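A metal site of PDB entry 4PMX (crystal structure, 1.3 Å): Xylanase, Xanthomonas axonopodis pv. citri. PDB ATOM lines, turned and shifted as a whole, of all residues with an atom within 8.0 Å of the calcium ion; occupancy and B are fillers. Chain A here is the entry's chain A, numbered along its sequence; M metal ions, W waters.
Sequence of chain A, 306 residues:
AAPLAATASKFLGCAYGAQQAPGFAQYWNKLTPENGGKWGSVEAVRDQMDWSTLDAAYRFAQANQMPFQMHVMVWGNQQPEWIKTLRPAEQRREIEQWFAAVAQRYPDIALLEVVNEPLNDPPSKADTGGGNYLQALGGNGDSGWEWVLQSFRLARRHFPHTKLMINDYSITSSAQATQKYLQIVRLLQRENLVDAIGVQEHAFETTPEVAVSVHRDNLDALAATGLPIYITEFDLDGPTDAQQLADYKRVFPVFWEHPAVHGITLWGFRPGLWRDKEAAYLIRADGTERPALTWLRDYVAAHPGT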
ATOM      1  N   TRP A  39      12.057 -20.826 -18.063  1.00  0.00           N
ATOM      2  CA  TRP A  39      11.988 -20.546 -19.470  1.00  0.00           C
ATOM      3  C   TRP A  39      11.883 -21.844 -20.313  1.00  0.00           C
ATOM      4  O   TRP A  39      11.103 -21.912 -21.299  1.00  0.00           O
ATOM      5  CB  TRP A  39      13.226 -19.798 -19.884  1.00  0.00           C
ATOM      6  CG  TRP A  39      13.234 -19.209 -21.271  1.00  0.00           C
ATOM      7  CD1 TRP A  39      12.178 -19.184 -22.178  1.00  0.00           C
ATOM      8  CD2 TRP A  39      14.324 -18.600 -21.949  1.00  0.00           C
ATOM      9  NE1 TRP A  39      12.547 -18.489 -23.331  1.00  0.00           N
ATOM     10  CE2 TRP A  39      13.855 -18.161 -23.231  1.00  0.00           C
ATOM     11  CE3 TRP A  39      15.659 -18.280 -21.556  1.00  0.00           C
ATOM     12  CZ2 TRP A  39      14.693 -17.414 -24.102  1.00  0.00           C
ATOM     13  CZ3 TRP A  39      16.470 -17.603 -22.403  1.00  0.00           C
ATOM     14  CH2 TRP A  39      16.007 -17.140 -23.645  1.00  0.00           C
ATOM     15  N   GLU A  43       9.104 -22.195 -23.287  1.00  0.00           N
ATOM     16  CA  GLU A  43       9.577 -22.177 -24.643  1.00  0.00           C
ATOM     17  C   GLU A  43      10.510 -23.360 -24.944  1.00  0.00           C
ATOM     18  O   GLU A  43      11.659 -23.207 -25.459  1.00  0.00           O
ATOM     19  CB  GLU A  43      10.208 -20.800 -24.943  1.00  0.00           C
ATOM     20  CG  GLU A  43      10.348 -20.463 -26.439  1.00  0.00           C
ATOM     21  CD  GLU A  43      10.879 -19.063 -26.770  1.00  0.00           C
ATOM     22  OE1 GLU A  43      11.119 -18.303 -25.836  1.00  0.00           O
ATOM     23  OE2 GLU A  43      11.098 -18.771 -27.982  1.00  0.00           O
ATOM     24  N   VAL A  45      10.085 -25.372 -27.341  1.00  0.00           N
ATOM     25  CA  VAL A  45      10.266 -25.300 -28.803  1.00  0.00           C
ATOM     26  C   VAL A  45      10.382 -23.810 -29.155  1.00  0.00           C
ATOM     27  O   VAL A  45       9.527 -23.029 -28.730  1.00  0.00           O
ATOM     28  CB  VAL A  45       9.094 -25.936 -29.550  1.00  0.00           C
ATOM     29  CG1 VAL A  45       9.245 -25.798 -31.046  1.00  0.00           C
ATOM     30  CG2 VAL A  45       8.961 -27.417 -29.133  1.00  0.00           C
ATOM     31  N   ARG A  46      11.446 -23.453 -29.879  1.00  0.00           N
ATOM     32  CA  ARG A  46      11.680 -22.062 -30.204  1.00  0.00           C
ATOM     33  C   ARG A  46      10.462 -21.382 -30.815  1.00  0.00           C
ATOM     34  O   ARG A  46       9.918 -21.848 -31.770  1.00  0.00           O
ATOM     35  CB  ARG A  46      12.918 -21.903 -31.085  1.00  0.00           C
ATOM     36  CG  ARG A  46      13.405 -20.503 -31.289  1.00  0.00           C
ATOM     37  CD  ARG A  46      14.516 -20.444 -32.328  1.00  0.00           C
ATOM     38  NE  ARG A  46      15.116 -19.188 -32.426  1.00  0.00           N
ATOM     39  CZ  ARG A  46      16.197 -18.924 -33.120  1.00  0.00           C
ATOM     40  NH1 ARG A  46      16.668 -19.849 -33.943  1.00  0.00           N
ATOM     41  NH2 ARG A  46      16.786 -17.778 -33.014  1.00  0.00           N
ATOM     42  N   ASP A  47      10.105 -20.218 -30.266  1.00  0.00           N
ATOM     43  CA  ASP A  47       9.064 -19.349 -30.782  1.00  0.00           C
ATOM     44  C   ASP A  47       7.633 -19.883 -30.711  1.00  0.00           C
ATOM     45  O   ASP A  47       6.727 -19.351 -31.378  1.00  0.00           O
ATOM     46  CB  ASP A  47       9.448 -18.829 -32.217  1.00  0.00           C
ATOM     47  CG  ASP A  47      10.636 -17.903 -32.199  1.00  0.00           C
ATOM     48  OD1 ASP A  47      11.080 -17.297 -31.114  1.00  0.00           O
ATOM     49  OD2 ASP A  47      11.223 -17.831 -33.283  1.00  0.00           O
ATOM     50  N   GLN A  48       7.436 -20.821 -29.829  1.00  0.00           N
ATOM     51  CA  GLN A  48       6.109 -21.180 -29.433  1.00  0.00           C
ATOM     52  C   GLN A  48       6.044 -21.257 -27.959  1.00  0.00           C
ATOM     53  O   GLN A  48       6.851 -21.888 -27.340  1.00  0.00           O
ATOM     54  CB  GLN A  48       5.584 -22.390 -30.148  1.00  0.00           C
ATOM     55  CG  GLN A  48       6.275 -23.733 -29.927  1.00  0.00           C
ATOM     56  CD  GLN A  48       5.742 -24.868 -30.852  1.00  0.00           C
ATOM     57  OE1 GLN A  48       5.735 -24.774 -32.091  1.00  0.00           O
ATOM     58  NE2 GLN A  48       5.347 -26.015 -30.220  1.00  0.00           N
ATOM     59  N   MET A  49       5.125 -20.500 -27.405  1.00  0.00           N
ATOM     60  CA  MET A  49       5.052 -20.214 -25.964  1.00  0.00           C
ATOM     61  C   MET A  49       3.933 -21.049 -25.399  1.00  0.00           C
ATOM     62  O   MET A  49       2.777 -20.932 -25.825  1.00  0.00           O
ATOM     63  CB  MET A  49       4.847 -18.718 -25.679  1.00  0.00           C
ATOM     64  CG  MET A  49       5.848 -17.766 -26.375  1.00  0.00           C
ATOM     65  SD  MET A  49       7.608 -18.175 -25.970  1.00  0.00           S
ATOM     66  CE  MET A  49       7.991 -16.963 -24.661  1.00  0.00           C
ATOM     67  N   TRP A  82      17.211 -25.425 -27.303  1.00  0.00           N
ATOM     68  CA  TRP A  82      17.644 -24.940 -28.612  1.00  0.00           C
ATOM     69  C   TRP A  82      18.542 -23.678 -28.573  1.00  0.00           C
ATOM     70  O   TRP A  82      19.216 -23.298 -29.528  1.00  0.00           O
ATOM     71  CB  TRP A  82      16.379 -24.687 -29.503  1.00  0.00           C
ATOM     72  CG  TRP A  82      15.378 -23.818 -28.765  1.00  0.00           C
ATOM     73  CD1 TRP A  82      14.297 -24.331 -28.079  1.00  0.00           C
ATOM     74  CD2 TRP A  82      15.410 -22.400 -28.531  1.00  0.00           C
ATOM     75  NE1 TRP A  82      13.604 -23.271 -27.447  1.00  0.00           N
ATOM     76  CE2 TRP A  82      14.289 -22.089 -27.695  1.00  0.00           C
ATOM     77  CE3 TRP A  82      16.222 -21.315 -28.980  1.00  0.00           C
ATOM     78  CZ2 TRP A  82      14.013 -20.788 -27.251  1.00  0.00           C
ATOM     79  CZ3 TRP A  82      15.920 -20.022 -28.488  1.00  0.00           C
ATOM     80  CH2 TRP A  82      14.832 -19.771 -27.660  1.00  0.00           C
ATOM     81  N   GLU A  90      22.152 -13.746 -31.152  1.00  0.00           N
ATOM     82  CA  GLU A  90      20.788 -14.324 -31.284  1.00  0.00           C
ATOM     83  C   GLU A  90      20.256 -14.786 -29.948  1.00  0.00           C
ATOM     84  O   GLU A  90      19.074 -14.616 -29.688  1.00  0.00           O
ATOM     85  CB  GLU A  90      20.758 -15.413 -32.371  1.00  0.00           C
ATOM     86  CG  GLU A  90      21.156 -14.960 -33.787  1.00  0.00           C
ATOM     87  CD  GLU A  90      20.183 -13.906 -34.394  1.00  0.00           C
ATOM     88  OE1 GLU A  90      19.085 -13.629 -33.821  1.00  0.00           O
ATOM     89  OE2 GLU A  90      20.577 -13.354 -35.452  1.00  0.00           O
ATOM     90  N   ARG A  93      18.798 -11.749 -28.201  1.00  0.00           N
ATOM     91  CA  ARG A  93      17.464 -11.369 -28.704  1.00  0.00           C
ATOM     92  C   ARG A  93      16.381 -12.271 -28.184  1.00  0.00           C
ATOM     93  O   ARG A  93      15.236 -11.867 -27.944  1.00  0.00           O
ATOM     94  CB  ARG A  93      17.379 -11.365 -30.240  1.00  0.00           C
ATOM     95  CG  ARG A  93      18.403 -10.372 -30.843  1.00  0.00           C
ATOM     96  CD  ARG A  93      18.493 -10.512 -32.326  1.00  0.00           C
ATOM     97  NE  ARG A  93      17.373  -9.993 -33.078  1.00  0.00           N
ATOM     98  CZ  ARG A  93      17.030 -10.296 -34.314  1.00  0.00           C
ATOM     99  NH1 ARG A  93      17.533 -11.341 -34.931  1.00  0.00           N
ATOM    100  NH2 ARG A  93      16.077  -9.611 -34.946  1.00  0.00           N
ATOM    101  N   GLU A  94      16.689 -13.553 -28.045  1.00  0.00           N
ATOM    102  CA  GLU A  94      15.716 -14.523 -27.457  1.00  0.00           C
ATOM    103  C   GLU A  94      15.432 -14.170 -25.980  1.00  0.00           C
ATOM    104  O   GLU A  94      14.298 -14.275 -25.522  1.00  0.00           O
ATOM    105  CB  GLU A  94      16.202 -15.970 -27.606  1.00  0.00           C
ATOM    106  CG  GLU A  94      16.221 -16.490 -29.042  1.00  0.00           C
ATOM    107  CD  GLU A  94      14.901 -16.624 -29.700  1.00  0.00           C
ATOM    108  OE1 GLU A  94      13.869 -16.507 -28.989  1.00  0.00           O
ATOM    109  OE2 GLU A  94      14.902 -16.874 -30.940  1.00  0.00           O
ATOM    110  N   ILE A  95      16.483 -13.806 -25.208  1.00  0.00           N
ATOM    111  CA  ILE A  95      16.307 -13.487 -23.788  1.00  0.00           C
ATOM    112  C   ILE A  95      15.425 -12.225 -23.701  1.00  0.00           C
ATOM    113  O   ILE A  95      14.485 -12.182 -22.897  1.00  0.00           O
ATOM    114  CB  ILE A  95      17.685 -13.269 -23.129  1.00  0.00           C
ATOM    115  CG1 ILE A  95      18.537 -14.536 -23.103  1.00  0.00           C
ATOM    116  CG2 ILE A  95      17.483 -12.768 -21.704  1.00  0.00           C
ATOM    117  CD1 ILE A  95      20.023 -14.319 -22.818  1.00  0.00           C
ATOM    118  N   GLU A  96      15.719 -11.223 -24.511  1.00  0.00           N
ATOM    119  CA  GLU A  96      14.952  -9.964 -24.483  1.00  0.00           C
ATOM    120  C   GLU A  96      13.485 -10.233 -24.846  1.00  0.00           C
ATOM    121  O   GLU A  96      12.566  -9.683 -24.216  1.00  0.00           O
ATOM    122  CB  GLU A  96      15.521  -8.929 -25.439  1.00  0.00           C
ATOM    123  CG  GLU A  96      14.862  -7.581 -25.127  1.00  0.00           C
ATOM    124  CD  GLU A  96      15.774  -6.348 -25.221  1.00  0.00           C
ATOM    125  OE1 GLU A  96      16.832  -6.445 -25.927  1.00  0.00           O
ATOM    126  OE2 GLU A  96      15.346  -5.244 -24.705  1.00  0.00           O
ATOM    127  N   GLN A  97      13.238 -11.114 -25.849  1.00  0.00           N
ATOM    128  CA  GLN A  97      11.866 -11.458 -26.254  1.00  0.00           C
ATOM    129  C   GLN A  97      11.094 -12.211 -25.152  1.00  0.00           C
ATOM    130  O   GLN A  97       9.912 -11.930 -24.882  1.00  0.00           O
ATOM    131  CB  GLN A  97      11.902 -12.341 -27.551  1.00  0.00           C
ATOM    132  CG  GLN A  97      10.517 -12.903 -27.903  1.00  0.00           C
ATOM    133  CD  GLN A  97      10.559 -13.361 -29.308  1.00  0.00           C
ATOM    134  OE1 GLN A  97      11.241 -14.351 -29.593  1.00  0.00           O
ATOM    135  NE2 GLN A  97       9.817 -12.714 -30.208  1.00  0.00           N
ATOM    136  N   TRP A  98      11.828 -13.085 -24.430  1.00  0.00           N
ATOM    137  CA  TRP A  98      11.245 -13.739 -23.210  1.00  0.00           C
ATOM    138  C   TRP A  98      10.874 -12.786 -22.121  1.00  0.00           C
ATOM    139  O   TRP A  98       9.743 -12.890 -21.548  1.00  0.00           O
ATOM    140  CB  TRP A  98      12.290 -14.817 -22.739  1.00  0.00           C
ATOM    141  CG  TRP A  98      12.260 -15.398 -21.403  1.00  0.00           C
ATOM    142  CD1 TRP A  98      13.320 -15.369 -20.494  1.00  0.00           C
ATOM    143  CD2 TRP A  98      11.200 -16.120 -20.747  1.00  0.00           C
ATOM    144  NE1 TRP A  98      12.990 -16.050 -19.338  1.00  0.00           N
ATOM    145  CE2 TRP A  98      11.699 -16.532 -19.445  1.00  0.00           C
ATOM    146  CE3 TRP A  98       9.910 -16.524 -21.115  1.00  0.00           C
ATOM    147  CZ2 TRP A  98      10.875 -17.240 -18.518  1.00  0.00           C
ATOM    148  CZ3 TRP A  98       9.120 -17.210 -20.218  1.00  0.00           C
ATOM    149  CH2 TRP A  98       9.610 -17.591 -18.934  1.00  0.00           C
ATOM    150  N   ALA A 101       7.810 -10.885 -23.307  1.00  0.00           N
ATOM    151  CA  ALA A 101       6.588 -11.749 -23.389  1.00  0.00           C
ATOM    152  C   ALA A 101       5.999 -11.871 -22.012  1.00  0.00           C
ATOM    153  O   ALA A 101       4.769 -11.776 -21.830  1.00  0.00           O
ATOM    154  CB  ALA A 101       6.991 -13.090 -23.969  1.00  0.00           C
HETATM  155 CA    CA M   1      11.530 -16.578 -28.923  1.00  0.00          CA
HETATM  156  O   HOH W   1       9.194 -16.428 -28.444  1.00  0.00           O
HETATM  157  O   HOH W   2      11.995 -15.802 -26.651  1.00  0.00           O
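The calcium ion is bound by OE1 of Glu 94 (2.3 Å), OE1 of Gln 97 (2.3 Å), OD1 of Asp 47 (2.3 Å), water W1 (2.4 Å), OE2 of Glu 43 (2.4 Å) and water W2 (2.4 Å).
Water W2 lies within hydrogen-bond range of OE1 of Glu 43 (2.8 Å) and O of Glu 94 (3.0 Å).
Of the 16 residues printed, 4 come within 4 Å of the calcium ion. The nearest printed residue that does not touch the calcium ion is Trp 82 (4.8 Å).
OE2 of Glu 94 is in salt-bridge range of NE of Arg 46 (2.8 Å). OE1 of Glu 43 sits at hydrogen-bond distance from NE1 of Trp 39 (2.9 Å). The indole nitrogen of Trp 82 lies within hydrogen-bond range of the backbone carbonyl oxygen of Glu 43 (2.8 Å).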
